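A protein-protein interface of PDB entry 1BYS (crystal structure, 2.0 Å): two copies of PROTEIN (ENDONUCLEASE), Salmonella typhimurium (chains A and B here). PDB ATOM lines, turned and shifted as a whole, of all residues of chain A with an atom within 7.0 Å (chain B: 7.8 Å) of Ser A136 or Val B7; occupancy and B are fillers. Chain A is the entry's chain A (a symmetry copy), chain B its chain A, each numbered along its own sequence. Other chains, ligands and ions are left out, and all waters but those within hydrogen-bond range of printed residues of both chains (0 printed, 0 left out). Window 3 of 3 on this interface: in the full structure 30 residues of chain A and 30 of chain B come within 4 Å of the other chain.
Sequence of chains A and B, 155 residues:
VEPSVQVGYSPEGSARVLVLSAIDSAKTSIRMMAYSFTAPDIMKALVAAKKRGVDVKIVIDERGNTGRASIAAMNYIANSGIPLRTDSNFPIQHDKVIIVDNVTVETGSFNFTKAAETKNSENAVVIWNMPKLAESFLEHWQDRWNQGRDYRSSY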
ATOM      1  N   ILE A  99       3.293 -13.550 -26.540  1.00  0.00           N
ATOM      2  CA  ILE A  99       2.098 -13.688 -25.702  1.00  0.00           C
ATOM      3  C   ILE A  99       1.127 -14.621 -26.415  1.00  0.00           C
ATOM      4  O   ILE A  99       0.654 -14.326 -27.521  1.00  0.00           O
ATOM      5  CB  ILE A  99       1.402 -12.330 -25.450  1.00  0.00           C
ATOM      6  CG1 ILE A  99       2.405 -11.322 -24.887  1.00  0.00           C
ATOM      7  CG2 ILE A  99       0.256 -12.510 -24.470  1.00  0.00           C
ATOM      8  CD1 ILE A  99       2.055  -9.889 -25.186  1.00  0.00           C
ATOM      9  N   ASN A 102      -3.632 -14.813 -25.054  1.00  0.00           N
ATOM     10  CA  ASN A 102      -3.912 -13.835 -24.010  1.00  0.00           C
ATOM     11  C   ASN A 102      -3.888 -14.316 -22.550  1.00  0.00           C
ATOM     12  O   ASN A 102      -4.483 -13.683 -21.666  1.00  0.00           O
ATOM     13  CB  ASN A 102      -5.244 -13.127 -24.290  1.00  0.00           C
ATOM     14  CG  ASN A 102      -5.189 -11.648 -23.937  1.00  0.00           C
ATOM     15  OD1 ASN A 102      -4.113 -11.105 -23.622  1.00  0.00           O
ATOM     16  ND2 ASN A 102      -6.335 -10.983 -23.990  1.00  0.00           N
ATOM     17  N   MET A 130      -1.757 -17.031 -16.773  1.00  0.00           N
ATOM     18  CA  MET A 130      -1.739 -15.935 -15.819  1.00  0.00           C
ATOM     19  C   MET A 130      -2.351 -14.814 -16.625  1.00  0.00           C
ATOM     20  O   MET A 130      -1.640 -13.936 -17.118  1.00  0.00           O
ATOM     21  CB  MET A 130      -0.313 -15.567 -15.419  1.00  0.00           C
ATOM     22  CG  MET A 130       0.355 -16.581 -14.503  1.00  0.00           C
ATOM     23  SD  MET A 130       1.521 -15.796 -13.379  1.00  0.00           S
ATOM     24  CE  MET A 130       2.569 -17.169 -12.988  1.00  0.00           C
ATOM     25  N   PRO A 131      -3.684 -14.845 -16.788  1.00  0.00           N
ATOM     26  CA  PRO A 131      -4.416 -13.828 -17.554  1.00  0.00           C
ATOM     27  C   PRO A 131      -3.985 -12.406 -17.224  1.00  0.00           C
ATOM     28  O   PRO A 131      -3.721 -11.618 -18.121  1.00  0.00           O
ATOM     29  CB  PRO A 131      -5.883 -14.102 -17.204  1.00  0.00           C
ATOM     30  CG  PRO A 131      -5.912 -15.581 -16.894  1.00  0.00           C
ATOM     31  CD  PRO A 131      -4.584 -15.871 -16.223  1.00  0.00           C
ATOM     32  N   LYS A 132      -3.893 -12.087 -15.938  1.00  0.00           N
ATOM     33  CA  LYS A 132      -3.496 -10.741 -15.523  1.00  0.00           C
ATOM     34  C   LYS A 132      -2.099 -10.358 -16.046  1.00  0.00           C
ATOM     35  O   LYS A 132      -1.874  -9.229 -16.492  1.00  0.00           O
ATOM     36  CB  LYS A 132      -3.520 -10.651 -13.992  1.00  0.00           C
ATOM     37  CG  LYS A 132      -4.816 -11.155 -13.360  1.00  0.00           C
ATOM     38  CD  LYS A 132      -4.994 -12.677 -13.553  1.00  0.00           C
ATOM     39  CE  LYS A 132      -3.915 -13.486 -12.824  1.00  0.00           C
ATOM     40  NZ  LYS A 132      -2.616 -13.530 -13.526  1.00  0.00           N
ATOM     41  N   LEU A 133      -1.157 -11.296 -15.980  1.00  0.00           N
ATOM     42  CA  LEU A 133       0.198 -11.038 -16.456  1.00  0.00           C
ATOM     43  C   LEU A 133       0.219 -10.835 -17.976  1.00  0.00           C
ATOM     44  O   LEU A 133       0.848  -9.893 -18.477  1.00  0.00           O
ATOM     45  CB  LEU A 133       1.131 -12.195 -16.073  1.00  0.00           C
ATOM     46  CG  LEU A 133       2.585 -12.027 -16.541  1.00  0.00           C
ATOM     47  CD1 LEU A 133       3.285 -10.930 -15.720  1.00  0.00           C
ATOM     48  CD2 LEU A 133       3.325 -13.364 -16.431  1.00  0.00           C
ATOM     49  N   ALA A 134      -0.474 -11.704 -18.712  1.00  0.00           N
ATOM     50  CA  ALA A 134      -0.511 -11.608 -20.173  1.00  0.00           C
ATOM     51  C   ALA A 134      -1.243 -10.352 -20.695  1.00  0.00           C
ATOM     52  O   ALA A 134      -0.866  -9.805 -21.740  1.00  0.00           O
ATOM     53  CB  ALA A 134      -1.129 -12.873 -20.761  1.00  0.00           C
ATOM     54  N   GLU A 135      -2.266  -9.879 -19.982  1.00  0.00           N
ATOM     55  CA  GLU A 135      -2.980  -8.676 -20.398  1.00  0.00           C
ATOM     56  C   GLU A 135      -2.072  -7.453 -20.185  1.00  0.00           C
ATOM     57  O   GLU A 135      -2.080  -6.506 -20.968  1.00  0.00           O
ATOM     58  CB  GLU A 135      -4.279  -8.528 -19.608  1.00  0.00           C
ATOM     59  CG  GLU A 135      -5.187  -7.383 -20.113  1.00  0.00           C
ATOM     60  CD  GLU A 135      -5.216  -7.214 -21.652  1.00  0.00           C
ATOM     61  OE1 GLU A 135      -4.300  -6.548 -22.205  1.00  0.00           O
ATOM     62  OE2 GLU A 135      -6.168  -7.731 -22.298  1.00  0.00           O
ATOM     63  N   SER A 136      -1.266  -7.480 -19.135  1.00  0.00           N
ATOM     64  CA  SER A 136      -0.332  -6.397 -18.895  1.00  0.00           C
ATOM     65  C   SER A 136       0.710  -6.406 -20.031  1.00  0.00           C
ATOM     66  O   SER A 136       1.069  -5.363 -20.584  1.00  0.00           O
ATOM     67  CB  SER A 136       0.360  -6.605 -17.540  1.00  0.00           C
ATOM     68  OG  SER A 136       1.553  -5.850 -17.472  1.00  0.00           O
ATOM     69  N   PHE A 137       1.205  -7.585 -20.394  1.00  0.00           N
ATOM     70  CA  PHE A 137       2.175  -7.671 -21.470  1.00  0.00           C
ATOM     71  C   PHE A 137       1.553  -7.202 -22.784  1.00  0.00           C
ATOM     72  O   PHE A 137       2.207  -6.524 -23.596  1.00  0.00           O
ATOM     73  CB  PHE A 137       2.689  -9.105 -21.605  1.00  0.00           C
ATOM     74  CG  PHE A 137       4.056  -9.321 -20.973  1.00  0.00           C
ATOM     75  CD1 PHE A 137       5.227  -9.059 -21.686  1.00  0.00           C
ATOM     76  CD2 PHE A 137       4.168  -9.807 -19.671  1.00  0.00           C
ATOM     77  CE1 PHE A 137       6.484  -9.284 -21.119  1.00  0.00           C
ATOM     78  CE2 PHE A 137       5.425 -10.036 -19.091  1.00  0.00           C
ATOM     79  CZ  PHE A 137       6.583  -9.773 -19.820  1.00  0.00           C
ATOM     80  N   LEU A 138       0.281  -7.542 -22.989  1.00  0.00           N
ATOM     81  CA  LEU A 138      -0.432  -7.154 -24.205  1.00  0.00           C
ATOM     82  C   LEU A 138      -0.456  -5.633 -24.372  1.00  0.00           C
ATOM     83  O   LEU A 138      -0.316  -5.123 -25.488  1.00  0.00           O
ATOM     84  CB  LEU A 138      -1.862  -7.705 -24.201  1.00  0.00           C
ATOM     85  CG  LEU A 138      -2.654  -7.260 -25.439  1.00  0.00           C
ATOM     86  CD1 LEU A 138      -1.979  -7.789 -26.708  1.00  0.00           C
ATOM     87  CD2 LEU A 138      -4.101  -7.742 -25.343  1.00  0.00           C
ATOM     88  N   GLU A 139      -0.627  -4.905 -23.271  1.00  0.00           N
ATOM     89  CA  GLU A 139      -0.619  -3.439 -23.326  1.00  0.00           C
ATOM     90  C   GLU A 139       0.764  -2.941 -23.781  1.00  0.00           C
ATOM     91  O   GLU A 139       0.885  -1.949 -24.507  1.00  0.00           O
ATOM     92  CB  GLU A 139      -0.951  -2.884 -21.946  1.00  0.00           C
ATOM     93  CG  GLU A 139      -2.269  -3.398 -21.394  1.00  0.00           C
ATOM     94  CD  GLU A 139      -2.713  -2.639 -20.148  1.00  0.00           C
ATOM     95  OE1 GLU A 139      -1.866  -1.961 -19.524  1.00  0.00           O
ATOM     96  OE2 GLU A 139      -3.908  -2.717 -19.787  1.00  0.00           O
ATOM     97  N   HIS A 140       1.804  -3.652 -23.347  1.00  0.00           N
ATOM     98  CA  HIS A 140       3.196  -3.363 -23.697  1.00  0.00           C
ATOM     99  C   HIS A 140       3.350  -3.602 -25.201  1.00  0.00           C
ATOM    100  O   HIS A 140       3.863  -2.758 -25.925  1.00  0.00           O
ATOM    101  CB  HIS A 140       4.110  -4.312 -22.911  1.00  0.00           C
ATOM    102  CG  HIS A 140       5.581  -4.057 -23.079  1.00  0.00           C
ATOM    103  ND1 HIS A 140       6.156  -2.819 -22.890  1.00  0.00           N
ATOM    104  CD2 HIS A 140       6.607  -4.909 -23.313  1.00  0.00           C
ATOM    105  CE1 HIS A 140       7.472  -2.918 -22.995  1.00  0.00           C
ATOM    106  NE2 HIS A 140       7.768  -4.179 -23.252  1.00  0.00           N
ATOM    107  N   TRP A 141       2.900  -4.769 -25.659  1.00  0.00           N
ATOM    108  CA  TRP A 141       2.966  -5.138 -27.070  1.00  0.00           C
ATOM    109  C   TRP A 141       2.198  -4.120 -27.924  1.00  0.00           C
ATOM    110  O   TRP A 141       2.701  -3.627 -28.944  1.00  0.00           O
ATOM    111  CB  TRP A 141       2.351  -6.546 -27.277  1.00  0.00           C
ATOM    112  CG  TRP A 141       2.307  -6.994 -28.736  1.00  0.00           C
ATOM    113  CD1 TRP A 141       3.256  -7.729 -29.399  1.00  0.00           C
ATOM    114  CD2 TRP A 141       1.309  -6.648 -29.729  1.00  0.00           C
ATOM    115  NE1 TRP A 141       2.918  -7.851 -30.731  1.00  0.00           N
ATOM    116  CE2 TRP A 141       1.735  -7.201 -30.960  1.00  0.00           C
ATOM    117  CE3 TRP A 141       0.109  -5.926 -29.691  1.00  0.00           C
ATOM    118  CZ2 TRP A 141       0.994  -7.049 -32.149  1.00  0.00           C
ATOM    119  CZ3 TRP A 141      -0.620  -5.779 -30.875  1.00  0.00           C
ATOM    120  CH2 TRP A 141      -0.171  -6.339 -32.079  1.00  0.00           C
ATOM    121  N   VAL B   5       3.836 -13.405  -9.825  1.00  0.00           N
ATOM    122  CA  VAL B   5       4.726 -12.797 -10.799  1.00  0.00           C
ATOM    123  C   VAL B   5       4.483 -11.310 -10.989  1.00  0.00           C
ATOM    124  O   VAL B   5       3.346 -10.859 -11.141  1.00  0.00           O
ATOM    125  CB  VAL B   5       4.599 -13.465 -12.206  1.00  0.00           C
ATOM    126  CG1 VAL B   5       5.626 -12.874 -13.148  1.00  0.00           C
ATOM    127  CG2 VAL B   5       4.777 -14.976 -12.106  1.00  0.00           C
ATOM    128  N   GLN B   6       5.563 -10.545 -10.974  1.00  0.00           N
ATOM    129  CA  GLN B   6       5.472  -9.113 -11.197  1.00  0.00           C
ATOM    130  C   GLN B   6       6.175  -8.835 -12.514  1.00  0.00           C
ATOM    131  O   GLN B   6       7.069  -9.583 -12.914  1.00  0.00           O
ATOM    132  CB  GLN B   6       6.191  -8.351 -10.100  1.00  0.00           C
ATOM    133  CG  GLN B   6       5.389  -8.197  -8.841  1.00  0.00           C
ATOM    134  CD  GLN B   6       6.120  -7.324  -7.861  1.00  0.00           C
ATOM    135  OE1 GLN B   6       6.967  -7.808  -7.113  1.00  0.00           O
ATOM    136  NE2 GLN B   6       5.820  -6.019  -7.870  1.00  0.00           N
ATOM    137  N   VAL B   7       5.784  -7.762 -13.180  1.00  0.00           N
ATOM    138  CA  VAL B   7       6.408  -7.396 -14.449  1.00  0.00           C
ATOM    139  C   VAL B   7       6.653  -5.890 -14.465  1.00  0.00           C
ATOM    140  O   VAL B   7       5.893  -5.113 -13.860  1.00  0.00           O
ATOM    141  CB  VAL B   7       5.495  -7.759 -15.666  1.00  0.00           C
ATOM    142  CG1 VAL B   7       4.144  -7.039 -15.531  1.00  0.00           C
ATOM    143  CG2 VAL B   7       6.187  -7.367 -16.981  1.00  0.00           C
ATOM    144  N   GLY B   8       7.716  -5.489 -15.145  1.00  0.00           N
ATOM    145  CA  GLY B   8       8.035  -4.081 -15.267  1.00  0.00           C
ATOM    146  C   GLY B   8       8.573  -3.822 -16.659  1.00  0.00           C
ATOM    147  O   GLY B   8       9.091  -4.740 -17.309  1.00  0.00           O
ATOM    148  N   TYR B   9       8.482  -2.585 -17.119  1.00  0.00           N
ATOM    149  CA  TYR B   9       8.953  -2.251 -18.466  1.00  0.00           C
ATOM    150  C   TYR B   9       9.848  -1.023 -18.561  1.00  0.00           C
ATOM    151  O   TYR B   9       9.853  -0.175 -17.670  1.00  0.00           O
ATOM    152  CB  TYR B   9       7.749  -2.022 -19.397  1.00  0.00           C
ATOM    153  CG  TYR B   9       6.679  -3.102 -19.318  1.00  0.00           C
ATOM    154  CD1 TYR B   9       6.852  -4.329 -19.962  1.00  0.00           C
ATOM    155  CD2 TYR B   9       5.503  -2.895 -18.605  1.00  0.00           C
ATOM    156  CE1 TYR B   9       5.876  -5.328 -19.886  1.00  0.00           C
ATOM    157  CE2 TYR B   9       4.524  -3.886 -18.521  1.00  0.00           C
ATOM    158  CZ  TYR B   9       4.713  -5.097 -19.157  1.00  0.00           C
ATOM    159  OH  TYR B   9       3.773  -6.108 -19.012  1.00  0.00           O
ATOM    160  N   SER B  14       9.269   1.139 -14.803  1.00  0.00           N
ATOM    161  CA  SER B  14       8.849   0.061 -13.928  1.00  0.00           C
ATOM    162  C   SER B  14       9.816  -1.131 -13.913  1.00  0.00           C
ATOM    163  O   SER B  14       9.924  -1.819 -12.902  1.00  0.00           O
ATOM    164  CB  SER B  14       7.449  -0.408 -14.324  1.00  0.00           C
ATOM    165  OG  SER B  14       7.344  -0.462 -15.732  1.00  0.00           O
ATOM    166  N   ALA B  15      10.523  -1.392 -15.010  1.00  0.00           N
ATOM    167  CA  ALA B  15      11.462  -2.525 -15.011  1.00  0.00           C
ATOM    168  C   ALA B  15      12.603  -2.277 -14.013  1.00  0.00           C
ATOM    169  O   ALA B  15      12.914  -3.123 -13.170  1.00  0.00           O
ATOM    170  CB  ALA B  15      12.049  -2.753 -16.417  1.00  0.00           C
ATOM    171  N   LEU B  18      11.469  -2.572 -10.442  1.00  0.00           N
ATOM    172  CA  LEU B  18      11.162  -3.961 -10.111  1.00  0.00           C
ATOM    173  C   LEU B  18      12.432  -4.769  -9.872  1.00  0.00           C
ATOM    174  O   LEU B  18      12.493  -5.578  -8.951  1.00  0.00           O
ATOM    175  CB  LEU B  18      10.342  -4.622 -11.235  1.00  0.00           C
ATOM    176  CG  LEU B  18       9.996  -6.105 -11.031  1.00  0.00           C
ATOM    177  CD1 LEU B  18       9.268  -6.336  -9.702  1.00  0.00           C
ATOM    178  CD2 LEU B  18       9.121  -6.563 -12.200  1.00  0.00           C
ATOM    179  N   THR B 107      14.080 -12.296 -14.474  1.00  0.00           N
ATOM    180  CA  THR B 107      14.615 -12.550 -15.806  1.00  0.00           C
ATOM    181  C   THR B 107      13.902 -11.656 -16.804  1.00  0.00           C
ATOM    182  O   THR B 107      13.046 -10.871 -16.421  1.00  0.00           O
ATOM    183  CB  THR B 107      14.516 -14.035 -16.239  1.00  0.00           C
ATOM    184  OG1 THR B 107      15.279 -14.209 -17.450  1.00  0.00           O
ATOM    185  CG2 THR B 107      13.048 -14.459 -16.452  1.00  0.00           C
ATOM    186  N   GLU B 122      11.959  -2.584 -22.924  1.00  0.00           N
ATOM    187  CA  GLU B 122      12.363  -3.820 -22.253  1.00  0.00           C
ATOM    188  C   GLU B 122      11.291  -4.331 -21.338  1.00  0.00           C
ATOM    189  O   GLU B 122      10.329  -3.640 -21.038  1.00  0.00           O
ATOM    190  CB  GLU B 122      13.610  -3.604 -21.367  1.00  0.00           C
ATOM    191  CG  GLU B 122      14.742  -2.819 -21.987  1.00  0.00           C
ATOM    192  CD  GLU B 122      15.758  -3.709 -22.646  1.00  0.00           C
ATOM    193  OE1 GLU B 122      15.479  -4.918 -22.854  1.00  0.00           O
ATOM    194  OE2 GLU B 122      16.837  -3.187 -22.965  1.00  0.00           O
ATOM    195  N   ASN B 123      11.478  -5.552 -20.869  1.00  0.00           N
ATOM    196  CA  ASN B 123      10.559  -6.134 -19.902  1.00  0.00           C
ATOM    197  C   ASN B 123      11.404  -6.910 -18.884  1.00  0.00           C
ATOM    198  O   ASN B 123      12.453  -7.485 -19.221  1.00  0.00           O
ATOM    199  CB  ASN B 123       9.552  -7.077 -20.577  1.00  0.00           C
ATOM    200  CG  ASN B 123      10.201  -8.327 -21.143  1.00  0.00           C
ATOM    201  OD1 ASN B 123      10.794  -8.296 -22.225  1.00  0.00           O
ATOM    202  ND2 ASN B 123      10.100  -9.429 -20.419  1.00  0.00           N
ATOM    203  N   ALA B 124      10.977  -6.884 -17.631  1.00  0.00           N
ATOM    204  CA  ALA B 124      11.653  -7.623 -16.580  1.00  0.00           C
ATOM    205  C   ALA B 124      10.540  -8.254 -15.768  1.00  0.00           C
ATOM    206  O   ALA B 124       9.527  -7.599 -15.477  1.00  0.00           O
ATOM    207  CB  ALA B 124      12.499  -6.680 -15.681  1.00  0.00           C
ATOM    208  N   VAL B 125      10.693  -9.530 -15.446  1.00  0.00           N
ATOM    209  CA  VAL B 125       9.701 -10.202 -14.635  1.00  0.00           C
ATOM    210  C   VAL B 125      10.373 -10.763 -13.397  1.00  0.00           C
ATOM    211  O   VAL B 125      11.561 -11.089 -13.403  1.00  0.00           O
ATOM    212  CB  VAL B 125       9.012 -11.377 -15.392  1.00  0.00           C
ATOM    213  CG1 VAL B 125       8.066 -10.832 -16.433  1.00  0.00           C
ATOM    214  CG2 VAL B 125      10.057 -12.289 -16.021  1.00  0.00           C
ATOM    215  N   VAL B 126       9.620 -10.841 -12.316  1.00  0.00           N
ATOM    216  CA  VAL B 126      10.148 -11.431 -11.107  1.00  0.00           C
ATOM    217  C   VAL B 126       9.129 -12.480 -10.733  1.00  0.00           C
ATOM    218  O   VAL B 126       7.976 -12.155 -10.439  1.00  0.00           O
ATOM    219  CB  VAL B 126      10.308 -10.406  -9.963  1.00  0.00           C
ATOM    220  CG1 VAL B 126      10.734 -11.123  -8.692  1.00  0.00           C
ATOM    221  CG2 VAL B 126      11.371  -9.386 -10.342  1.00  0.00           C
ATOM    222  N   ILE B 127       9.547 -13.741 -10.812  1.00  0.00           N
ATOM    223  CA  ILE B 127       8.701 -14.869 -10.462  1.00  0.00           C
ATOM    224  C   ILE B 127       9.011 -15.222  -9.007  1.00  0.00           C
ATOM    225  O   ILE B 127      10.031 -15.862  -8.707  1.00  0.00           O
ATOM    226  CB  ILE B 127       9.008 -16.078 -11.359  1.00  0.00           C
ATOM    227  CG1 ILE B 127       8.652 -15.756 -12.819  1.00  0.00           C
ATOM    228  CG2 ILE B 127       8.208 -17.279 -10.889  1.00  0.00           C
ATOM    229  CD1 ILE B 127       9.605 -16.357 -13.857  1.00  0.00           C
ATOM    230  N   TRP B 128       8.135 -14.797  -8.100  1.00  0.00           N
ATOM    231  CA  TRP B 128       8.328 -15.049  -6.672  1.00  0.00           C
ATOM    232  C   TRP B 128       7.911 -16.416  -6.146  1.00  0.00           C
ATOM    233  O   TRP B 128       6.852 -16.935  -6.498  1.00  0.00           O
ATOM    234  CB  TRP B 128       7.575 -14.016  -5.836  1.00  0.00           C
ATOM    235  CG  TRP B 128       7.919 -12.621  -6.132  1.00  0.00           C
ATOM    236  CD1 TRP B 128       7.284 -11.787  -7.006  1.00  0.00           C
ATOM    237  CD2 TRP B 128       8.946 -11.842  -5.502  1.00  0.00           C
ATOM    238  NE1 TRP B 128       7.857 -10.535  -6.957  1.00  0.00           N
ATOM    239  CE2 TRP B 128       8.874 -10.548  -6.043  1.00  0.00           C
ATOM    240  CE3 TRP B 128       9.918 -12.126  -4.537  1.00  0.00           C
ATOM    241  CZ2 TRP B 128       9.749  -9.525  -5.645  1.00  0.00           C
ATOM    242  CZ3 TRP B 128      10.773 -11.112  -4.147  1.00  0.00           C
ATOM    243  CH2 TRP B 128      10.686  -9.832  -4.695  1.00  0.00           C
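OG of Ser A136 is in hydrogen-bond range of OH of Tyr B9, 2.7 Å away.
N of Phe A137 lies within hydrogen-bond range of OH of Tyr B9 (3.3 Å).
NE2 of His A140 is in hydrogen-bond range of O of Glu B122, at 3.4 Å.
The side-chain hydroxyl (OG) of Ser B14 is in hydrogen-bond range of the backbone NH (N) of Tyr B9, at 2.8 Å.
The backbone carbonyl oxygen (O) of Tyr B9 is in hydrogen-bond range of the backbone NH (N) of Ala B15, 3.0 Å away.
O of Thr B107 lies within hydrogen-bond range of N of Val B125.
Among the printed residues, merely in contact across the chains: Met A130 with Val B5, Leu A133 with Val B5, Leu A133 with Val B7, Ser A136 with Val B7, Phe A137 with Val B7, Phe A137 with Asn B123, Phe A137 with Val B125 and His A140 with Tyr B9.
Of the printed residues of chain B, Leu A133 touches Val B5 and Val B7.
Printed residues of chain B within 4 Å of Phe A137: Val B7, Tyr B9, Asn B123 and Val B125.
Val B7 touches just these residues of chain A: Leu A133 (3.9 Å), Ser A136 (3.4 Å) and Phe A137 (3.5 Å).
Ala B15 touches none of the printed residues of chain A.
Leu B18 touches none of the printed residues of chain A.
Of the printed residues of chain A, Asn B123 touches Phe A137 (3.6 Å).
The nearest residue of chain B that does not touch Ser A136 is Gly B8 (6.6 Å).
Hydrophobic or aromatic side chains of chain B within 4 Å of the printed part of chain A: Val B5, Val B7, Tyr B9 and Val B125.
Of the 14 printed residues of chain A, 5 touch a printed residue of chain B.
Hydrophobic or aromatic side chains of chain A within 4 Å of the printed part of chain B: Met A130, Leu A133, Phe A137 and His A140.
Among the printed residues, 11 pairs touch across the chains.
Among the printed residues, no Asp or Glu carboxylate lies within 4 Å of a Lys or Arg side-chain nitrogen of the other chain.
No position is printed for both chains.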
